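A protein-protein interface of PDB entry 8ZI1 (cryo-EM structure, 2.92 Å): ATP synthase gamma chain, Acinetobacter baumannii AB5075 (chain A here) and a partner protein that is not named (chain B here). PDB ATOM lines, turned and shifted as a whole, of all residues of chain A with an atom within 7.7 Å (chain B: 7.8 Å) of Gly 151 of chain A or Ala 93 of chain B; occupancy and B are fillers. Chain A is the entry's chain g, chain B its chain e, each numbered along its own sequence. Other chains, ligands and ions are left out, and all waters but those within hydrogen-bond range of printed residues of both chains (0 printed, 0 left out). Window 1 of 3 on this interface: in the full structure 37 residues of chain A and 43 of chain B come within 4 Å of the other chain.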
ATOM      1  N   ILE A 118       3.013  10.529   0.719  1.00  0.00           N
ATOM      2  CA  ILE A 118       4.314   9.897   0.527  1.00  0.00           C
ATOM      3  C   ILE A 118       5.231  10.288   1.679  1.00  0.00           C
ATOM      4  O   ILE A 118       6.163   9.554   2.026  1.00  0.00           O
ATOM      5  CB  ILE A 118       4.931  10.283  -0.830  1.00  0.00           C
ATOM      6  CG1 ILE A 118       3.912  10.092  -1.954  1.00  0.00           C
ATOM      7  CG2 ILE A 118       6.173   9.456  -1.112  1.00  0.00           C
ATOM      8  CD1 ILE A 118       3.478   8.656  -2.142  1.00  0.00           C
ATOM      9  N   GLY A 135      -3.404   5.728  -0.410  1.00  0.00           N
ATOM     10  CA  GLY A 135      -2.098   5.092  -0.150  1.00  0.00           C
ATOM     11  C   GLY A 135      -1.111   5.955   0.615  1.00  0.00           C
ATOM     12  O   GLY A 135      -1.041   7.161   0.334  1.00  0.00           O
ATOM     13  N   THR A 137       3.029   5.640   1.635  1.00  0.00           N
ATOM     14  CA  THR A 137       4.315   4.895   1.679  1.00  0.00           C
ATOM     15  C   THR A 137       5.343   5.806   2.345  1.00  0.00           C
ATOM     16  O   THR A 137       5.484   6.937   1.878  1.00  0.00           O
ATOM     17  CB  THR A 137       4.734   4.463   0.270  1.00  0.00           C
ATOM     18  OG1 THR A 137       4.738   5.626  -0.558  1.00  0.00           O
ATOM     19  CG2 THR A 137       3.812   3.422  -0.324  1.00  0.00           C
ATOM     20  N   LEU A 146      12.431   3.633  -7.790  1.00  0.00           N
ATOM     21  CA  LEU A 146      11.083   3.522  -8.335  1.00  0.00           C
ATOM     22  C   LEU A 146      10.303   2.401  -7.660  1.00  0.00           C
ATOM     23  O   LEU A 146       9.114   2.558  -7.358  1.00  0.00           O
ATOM     24  CB  LEU A 146      11.145   3.300  -9.846  1.00  0.00           C
ATOM     25  CG  LEU A 146      10.939   4.549 -10.705  1.00  0.00           C
ATOM     26  CD1 LEU A 146      10.972   4.200 -12.182  1.00  0.00           C
ATOM     27  CD2 LEU A 146       9.633   5.234 -10.340  1.00  0.00           C
ATOM     28  N   GLU A 147      10.952   1.250  -7.524  1.00  0.00           N
ATOM     29  CA  GLU A 147      10.283   0.113  -6.861  1.00  0.00           C
ATOM     30  C   GLU A 147       9.581   0.657  -5.617  1.00  0.00           C
ATOM     31  O   GLU A 147       8.446   0.232  -5.344  1.00  0.00           O
ATOM     32  CB  GLU A 147      11.318  -0.955  -6.514  1.00  0.00           C
ATOM     33  CG  GLU A 147      11.978  -1.574  -7.734  1.00  0.00           C
ATOM     34  CD  GLU A 147      13.218  -0.862  -8.250  1.00  0.00           C
ATOM     35  OE1 GLU A 147      13.433   0.305  -7.868  1.00  0.00           O
ATOM     36  OE2 GLU A 147      13.967  -1.477  -9.034  1.00  0.00           O
ATOM     37  N   GLN A 148      10.233   1.579  -4.909  1.00  0.00           N
ATOM     38  CA  GLN A 148       9.657   2.089  -3.638  1.00  0.00           C
ATOM     39  C   GLN A 148       8.345   2.838  -3.891  1.00  0.00           C
ATOM     40  O   GLN A 148       7.404   2.643  -3.102  1.00  0.00           O
ATOM     41  CB  GLN A 148      10.681   2.973  -2.922  1.00  0.00           C
ATOM     42  CG  GLN A 148      12.080   2.376  -2.912  1.00  0.00           C
ATOM     43  CD  GLN A 148      13.059   3.233  -2.149  1.00  0.00           C
ATOM     44  OE1 GLN A 148      12.678   4.159  -1.439  1.00  0.00           O
ATOM     45  NE2 GLN A 148      14.337   2.925  -2.288  1.00  0.00           N
ATOM     46  N   LEU A 149       8.278   3.666  -4.934  1.00  0.00           N
ATOM     47  CA  LEU A 149       7.059   4.501  -5.118  1.00  0.00           C
ATOM     48  C   LEU A 149       6.194   3.995  -6.275  1.00  0.00           C
ATOM     49  O   LEU A 149       5.172   4.647  -6.554  1.00  0.00           O
ATOM     50  CB  LEU A 149       7.495   5.950  -5.354  1.00  0.00           C
ATOM     51  CG  LEU A 149       8.341   6.194  -6.603  1.00  0.00           C
ATOM     52  CD1 LEU A 149       7.461   6.268  -7.840  1.00  0.00           C
ATOM     53  CD2 LEU A 149       9.153   7.470  -6.459  1.00  0.00           C
ATOM     54  N   THR A 150       6.551   2.873  -6.901  1.00  0.00           N
ATOM     55  CA  THR A 150       5.790   2.442  -8.104  1.00  0.00           C
ATOM     56  C   THR A 150       4.327   2.183  -7.738  1.00  0.00           C
ATOM     57  O   THR A 150       3.436   2.638  -8.479  1.00  0.00           O
ATOM     58  CB  THR A 150       6.413   1.181  -8.711  1.00  0.00           C
ATOM     59  OG1 THR A 150       7.658   1.554  -9.303  1.00  0.00           O
ATOM     60  CG2 THR A 150       5.533   0.519  -9.747  1.00  0.00           C
ATOM     61  N   GLY A 151       4.093   1.482  -6.632  1.00  0.00           N
ATOM     62  CA  GLY A 151       2.715   1.150  -6.232  1.00  0.00           C
ATOM     63  C   GLY A 151       1.904   2.368  -5.844  1.00  0.00           C
ATOM     64  O   GLY A 151       0.731   2.446  -6.258  1.00  0.00           O
ATOM     65  N   SER A 152       2.506   3.311  -5.118  1.00  0.00           N
ATOM     66  CA  SER A 152       1.713   4.449  -4.586  1.00  0.00           C
ATOM     67  C   SER A 152       1.083   5.259  -5.720  1.00  0.00           C
ATOM     68  O   SER A 152      -0.107   5.599  -5.617  1.00  0.00           O
ATOM     69  CB  SER A 152       2.577   5.322  -3.726  1.00  0.00           C
ATOM     70  OG  SER A 152       3.784   5.649  -4.397  1.00  0.00           O
ATOM     71  N   VAL A 153       1.856   5.552  -6.761  1.00  0.00           N
ATOM     72  CA  VAL A 153       1.290   6.297  -7.920  1.00  0.00           C
ATOM     73  C   VAL A 153       0.247   5.422  -8.620  1.00  0.00           C
ATOM     74  O   VAL A 153      -0.817   5.960  -8.989  1.00  0.00           O
ATOM     75  CB  VAL A 153       2.388   6.780  -8.887  1.00  0.00           C
ATOM     76  CG1 VAL A 153       3.306   5.659  -9.346  1.00  0.00           C
ATOM     77  CG2 VAL A 153       1.815   7.533 -10.076  1.00  0.00           C
ATOM     78  N   GLN A 154       0.508   4.118  -8.747  1.00  0.00           N
ATOM     79  CA  GLN A 154      -0.409   3.266  -9.551  1.00  0.00           C
ATOM     80  C   GLN A 154      -1.821   3.262  -8.958  1.00  0.00           C
ATOM     81  O   GLN A 154      -2.778   3.436  -9.737  1.00  0.00           O
ATOM     82  CB  GLN A 154       0.152   1.846  -9.623  1.00  0.00           C
ATOM     83  CG  GLN A 154      -0.162   1.131 -10.929  1.00  0.00           C
ATOM     84  CD  GLN A 154       0.478  -0.234 -10.974  1.00  0.00           C
ATOM     85  OE1 GLN A 154       0.835  -0.802  -9.946  1.00  0.00           O
ATOM     86  NE2 GLN A 154       0.631  -0.772 -12.172  1.00  0.00           N
ATOM     87  N   VAL A 155      -1.950   3.099  -7.640  1.00  0.00           N
ATOM     88  CA  VAL A 155      -3.313   2.987  -7.037  1.00  0.00           C
ATOM     89  C   VAL A 155      -4.055   4.313  -7.227  1.00  0.00           C
ATOM     90  O   VAL A 155      -5.255   4.278  -7.555  1.00  0.00           O
ATOM     91  CB  VAL A 155      -3.266   2.560  -5.558  1.00  0.00           C
ATOM     92  CG1 VAL A 155      -3.017   1.067  -5.419  1.00  0.00           C
ATOM     93  CG2 VAL A 155      -2.246   3.350  -4.756  1.00  0.00           C
ATOM     94  N   MET A 156      -3.360   5.432  -7.044  1.00  0.00           N
ATOM     95  CA  MET A 156      -4.028   6.753  -7.136  1.00  0.00           C
ATOM     96  C   MET A 156      -4.611   6.928  -8.538  1.00  0.00           C
ATOM     97  O   MET A 156      -5.729   7.458  -8.648  1.00  0.00           O
ATOM     98  CB  MET A 156      -3.019   7.872  -6.870  1.00  0.00           C
ATOM     99  CG  MET A 156      -3.640   9.252  -6.818  1.00  0.00           C
ATOM    100  SD  MET A 156      -3.953   9.796  -5.121  1.00  0.00           S
ATOM    101  CE  MET A 156      -5.491  10.687  -5.350  1.00  0.00           C
ATOM    102  N   LEU A 157      -3.884   6.495  -9.568  1.00  0.00           N
ATOM    103  CA  LEU A 157      -4.339   6.722 -10.933  1.00  0.00           C
ATOM    104  C   LEU A 157      -5.325   5.654 -11.397  1.00  0.00           C
ATOM    105  O   LEU A 157      -6.149   5.922 -12.275  1.00  0.00           O
ATOM    106  CB  LEU A 157      -3.136   6.811 -11.876  1.00  0.00           C
ATOM    107  CG  LEU A 157      -3.380   7.238 -13.326  1.00  0.00           C
ATOM    108  CD1 LEU A 157      -2.153   7.938 -13.842  1.00  0.00           C
ATOM    109  CD2 LEU A 157      -3.687   6.047 -14.218  1.00  0.00           C
ATOM    110  N   ARG B  85       9.420  -4.657 -15.524  1.00  0.00           N
ATOM    111  CA  ARG B  85       8.060  -4.160 -15.392  1.00  0.00           C
ATOM    112  C   ARG B  85       7.388  -3.883 -16.729  1.00  0.00           C
ATOM    113  O   ARG B  85       6.266  -3.366 -16.737  1.00  0.00           O
ATOM    114  CB  ARG B  85       8.037  -2.881 -14.533  1.00  0.00           C
ATOM    115  CG  ARG B  85       8.869  -1.729 -15.088  1.00  0.00           C
ATOM    116  CD  ARG B  85       8.014  -0.764 -15.898  1.00  0.00           C
ATOM    117  NE  ARG B  85       8.779   0.370 -16.401  1.00  0.00           N
ATOM    118  CZ  ARG B  85       8.313   1.264 -17.261  1.00  0.00           C
ATOM    119  NH1 ARG B  85       7.079   1.190 -17.734  1.00  0.00           N
ATOM    120  NH2 ARG B  85       9.102   2.259 -17.657  1.00  0.00           N
ATOM    121  N   ASN B  88       3.511  -4.533 -18.046  1.00  0.00           N
ATOM    122  CA  ASN B  88       2.367  -3.757 -17.569  1.00  0.00           C
ATOM    123  C   ASN B  88       1.679  -4.459 -16.398  1.00  0.00           C
ATOM    124  O   ASN B  88       0.452  -4.572 -16.341  1.00  0.00           O
ATOM    125  CB  ASN B  88       1.378  -3.479 -18.705  1.00  0.00           C
ATOM    126  CG  ASN B  88       0.400  -2.369 -18.371  1.00  0.00           C
ATOM    127  OD1 ASN B  88       0.535  -1.694 -17.351  1.00  0.00           O
ATOM    128  ND2 ASN B  88      -0.594  -2.178 -19.230  1.00  0.00           N
ATOM    129  N   LEU B  89       2.489  -4.945 -15.460  1.00  0.00           N
ATOM    130  CA  LEU B  89       1.950  -5.619 -14.286  1.00  0.00           C
ATOM    131  C   LEU B  89       1.173  -4.628 -13.426  1.00  0.00           C
ATOM    132  O   LEU B  89       1.623  -3.503 -13.191  1.00  0.00           O
ATOM    133  CB  LEU B  89       3.075  -6.273 -13.480  1.00  0.00           C
ATOM    134  CG  LEU B  89       3.948  -5.435 -12.539  1.00  0.00           C
ATOM    135  CD1 LEU B  89       4.732  -6.336 -11.598  1.00  0.00           C
ATOM    136  CD2 LEU B  89       4.891  -4.523 -13.312  1.00  0.00           C
ATOM    137  N   ASP B  90      -0.013  -5.038 -12.985  1.00  0.00           N
ATOM    138  CA  ASP B  90      -0.858  -4.195 -12.151  1.00  0.00           C
ATOM    139  C   ASP B  90      -1.123  -4.802 -10.784  1.00  0.00           C
ATOM    140  O   ASP B  90      -0.882  -4.145  -9.764  1.00  0.00           O
ATOM    141  CB  ASP B  90      -2.187  -3.911 -12.868  1.00  0.00           C
ATOM    142  CG  ASP B  90      -2.080  -2.770 -13.860  1.00  0.00           C
ATOM    143  OD1 ASP B  90      -1.174  -1.925 -13.698  1.00  0.00           O
ATOM    144  OD2 ASP B  90      -2.898  -2.719 -14.802  1.00  0.00           O
ATOM    145  N   GLU B  91      -1.609  -6.044 -10.730  1.00  0.00           N
ATOM    146  CA  GLU B  91      -1.934  -6.658  -9.447  1.00  0.00           C
ATOM    147  C   GLU B  91      -0.688  -6.858  -8.594  1.00  0.00           C
ATOM    148  O   GLU B  91      -0.695  -6.563  -7.394  1.00  0.00           O
ATOM    149  CB  GLU B  91      -2.649  -7.991  -9.668  1.00  0.00           C
ATOM    150  CG  GLU B  91      -3.051  -8.700  -8.386  1.00  0.00           C
ATOM    151  CD  GLU B  91      -4.138  -7.964  -7.627  1.00  0.00           C
ATOM    152  OE1 GLU B  91      -4.940  -7.256  -8.272  1.00  0.00           O
ATOM    153  OE2 GLU B  91      -4.188  -8.091  -6.385  1.00  0.00           O
ATOM    154  N   ALA B  92       0.393  -7.361  -9.196  1.00  0.00           N
ATOM    155  CA  ALA B  92       1.618  -7.598  -8.440  1.00  0.00           C
ATOM    156  C   ALA B  92       2.213  -6.294  -7.926  1.00  0.00           C
ATOM    157  O   ALA B  92       2.712  -6.234  -6.797  1.00  0.00           O
ATOM    158  CB  ALA B  92       2.631  -8.349  -9.302  1.00  0.00           C
ATOM    159  N   ALA B  93       2.168  -5.239  -8.740  1.00  0.00           N
ATOM    160  CA  ALA B  93       2.731  -3.955  -8.342  1.00  0.00           C
ATOM    161  C   ALA B  93       1.863  -3.216  -7.333  1.00  0.00           C
ATOM    162  O   ALA B  93       2.300  -2.194  -6.794  1.00  0.00           O
ATOM    163  CB  ALA B  93       2.959  -3.080  -9.575  1.00  0.00           C
ATOM    164  N   ILE B  94       0.648  -3.695  -7.071  1.00  0.00           N
ATOM    165  CA  ILE B  94      -0.206  -3.130  -6.032  1.00  0.00           C
ATOM    166  C   ILE B  94      -0.428  -4.094  -4.882  1.00  0.00           C
ATOM    167  O   ILE B  94      -1.156  -3.756  -3.937  1.00  0.00           O
ATOM    168  CB  ILE B  94      -1.557  -2.658  -6.600  1.00  0.00           C
ATOM    169  CG1 ILE B  94      -2.415  -3.854  -7.016  1.00  0.00           C
ATOM    170  CG2 ILE B  94      -1.342  -1.701  -7.765  1.00  0.00           C
ATOM    171  CD1 ILE B  94      -3.839  -3.490  -7.370  1.00  0.00           C
ATOM    172  N   LEU B  95       0.162  -5.291  -4.932  1.00  0.00           N
ATOM    173  CA  LEU B  95       0.092  -6.191  -3.785  1.00  0.00           C
ATOM    174  C   LEU B  95       0.739  -5.564  -2.559  1.00  0.00           C
ATOM    175  O   LEU B  95       0.190  -5.633  -1.452  1.00  0.00           O
ATOM    176  CB  LEU B  95       0.757  -7.527  -4.114  1.00  0.00           C
ATOM    177  CG  LEU B  95      -0.023  -8.494  -5.004  1.00  0.00           C
ATOM    178  CD1 LEU B  95       0.822  -9.710  -5.351  1.00  0.00           C
ATOM    179  CD2 LEU B  95      -1.323  -8.911  -4.332  1.00  0.00           C
ATOM    180  N   GLU B  96       1.908  -4.945  -2.733  1.00  0.00           N
ATOM    181  CA  GLU B  96       2.529  -4.231  -1.624  1.00  0.00           C
ATOM    182  C   GLU B  96       1.720  -3.001  -1.236  1.00  0.00           C
ATOM    183  O   GLU B  96       1.707  -2.617  -0.062  1.00  0.00           O
ATOM    184  CB  GLU B  96       3.968  -3.847  -1.977  1.00  0.00           C
ATOM    185  CG  GLU B  96       4.101  -2.766  -3.038  1.00  0.00           C
ATOM    186  CD  GLU B  96       4.125  -3.325  -4.447  1.00  0.00           C
ATOM    187  OE1 GLU B  96       3.667  -4.470  -4.648  1.00  0.00           O
ATOM    188  OE2 GLU B  96       4.615  -2.620  -5.354  1.00  0.00           O
ATOM    189  N   ALA B  97       1.036  -2.379  -2.200  1.00  0.00           N
ATOM    190  CA  ALA B  97       0.166  -1.254  -1.876  1.00  0.00           C
ATOM    191  C   ALA B  97      -0.962  -1.688  -0.953  1.00  0.00           C
ATOM    192  O   ALA B  97      -1.317  -0.971  -0.010  1.00  0.00           O
ATOM    193  CB  ALA B  97      -0.392  -0.635  -3.157  1.00  0.00           C
ATOM    194  N   ARG B  98      -1.535  -2.867  -1.204  1.00  0.00           N
ATOM    195  CA  ARG B  98      -2.564  -3.398  -0.321  1.00  0.00           C
ATOM    196  C   ARG B  98      -2.040  -3.641   1.088  1.00  0.00           C
ATOM    197  O   ARG B  98      -2.834  -3.701   2.033  1.00  0.00           O
ATOM    198  CB  ARG B  98      -3.132  -4.695  -0.901  1.00  0.00           C
ATOM    199  CG  ARG B  98      -3.838  -4.514  -2.235  1.00  0.00           C
ATOM    200  CD  ARG B  98      -5.158  -3.781  -2.070  1.00  0.00           C
ATOM    201  NE  ARG B  98      -5.889  -3.685  -3.327  1.00  0.00           N
ATOM    202  CZ  ARG B  98      -5.796  -2.667  -4.172  1.00  0.00           C
ATOM    203  NH1 ARG B  98      -5.003  -1.636  -3.927  1.00  0.00           N
ATOM    204  NH2 ARG B  98      -6.515  -2.684  -5.290  1.00  0.00           N
ATOM    205  N   ALA B 101       0.558   0.667   1.387  1.00  0.00           N
ATOM    206  CA  ALA B 101       0.007   1.979   1.064  1.00  0.00           C
ATOM    207  C   ALA B 101      -1.133   2.360   2.006  1.00  0.00           C
ATOM    208  O   ALA B 101      -1.045   3.360   2.722  1.00  0.00           O
ATOM    209  CB  ALA B 101      -0.462   2.011  -0.395  1.00  0.00           C
ATOM    210  N   GLU B 102      -2.204   1.569   2.020  1.00  0.00           N
ATOM    211  CA  GLU B 102      -3.349   1.864   2.871  1.00  0.00           C
ATOM    212  C   GLU B 102      -3.384   1.039   4.148  1.00  0.00           C
ATOM    213  O   GLU B 102      -3.948   1.495   5.146  1.00  0.00           O
ATOM    214  CB  GLU B 102      -4.658   1.657   2.098  1.00  0.00           C
ATOM    215  CG  GLU B 102      -4.919   0.226   1.668  1.00  0.00           C
ATOM    216  CD  GLU B 102      -4.403  -0.063   0.273  1.00  0.00           C
ATOM    217  OE1 GLU B 102      -3.581   0.728  -0.234  1.00  0.00           O
ATOM    218  OE2 GLU B 102      -4.826  -1.077  -0.319  1.00  0.00           O
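O of Leu 89 of chain B sits at hydrogen-bond distance from NE2 of Gln 154 of chain A (3.1 Å). OD1 of Asp 90 of chain B is in hydrogen-bond range of NE2 of Gln 154 of chain A.
NH1 of Arg 98 of chain B is in salt-bridge range of OE2 of Glu 102 of chain B (3.7 Å). The backbone NH (N) of Glu 102 of chain B sits close to the backbone carbonyl oxygen (O) of Ala 97 of chain B, at 3.4 Å.
Among the printed residues, pairs that only touch across the chains: Gln 154 of chain A with Ala 93 of chain B (3.1 Å), Gln 154 of chain A with Ile 94 of chain B (3.2 Å), Gly 135 of chain A with Ala 101 of chain B (3.3 Å), Gly 151 of chain A with Ala 93 of chain B (3.4 Å), Val 155 of chain A with Arg 98 of chain B (3.7 Å), Val 155 of chain A with Ala 97 of chain B (3.9 Å) and Val 155 of chain A with Ile 94 of chain B (3.996 Å).
Ile 118 of chain A touches none of the printed residues of chain B. Of chain B, only Ala 93 (3.4 Å) comes within 4 Å of Gly 151 of chain A. Of the printed residues of chain B, Val 155 of chain A touches Ile 94 (3.996 Å), Ala 97 (3.9 Å) and Arg 98 (3.7 Å). Met 156 of chain A touches none of the printed residues of chain B. Of the printed residues of chain A, Asp 90 of chain B touches Gln 154. Ala 93 of chain B touches two residues of chain A. Of the printed residues of chain A, Ile 94 of chain B touches Gln 154 (3.2 Å) and Val 155 (3.996 Å). Printed residues of chain A within 4 Å of Arg 98 of chain B: Val 155. The nearest residue of chain B that does not touch Gly 151 of chain A is Glu 96 of chain B (4.3 Å). The nearest printed residue of chain B that does not touch Gly 135 of chain A is Glu 102 of chain B (4.1 Å).
Of the 14 printed residues of chain B, 7 touch a printed residue of chain A. Printed residues of chain B that touch a printed residue of chain A: Leu 89, Asp 90, Ala 93, Ile 94, Ala 97, Arg 98 and Ala 101. Along chain B the printed residues that touch a printed residue of chain A span positions 89 to 101. Printed residues of chain A that touch a printed residue of chain B: Gly 135, Gly 151, Gln 154 and Val 155.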
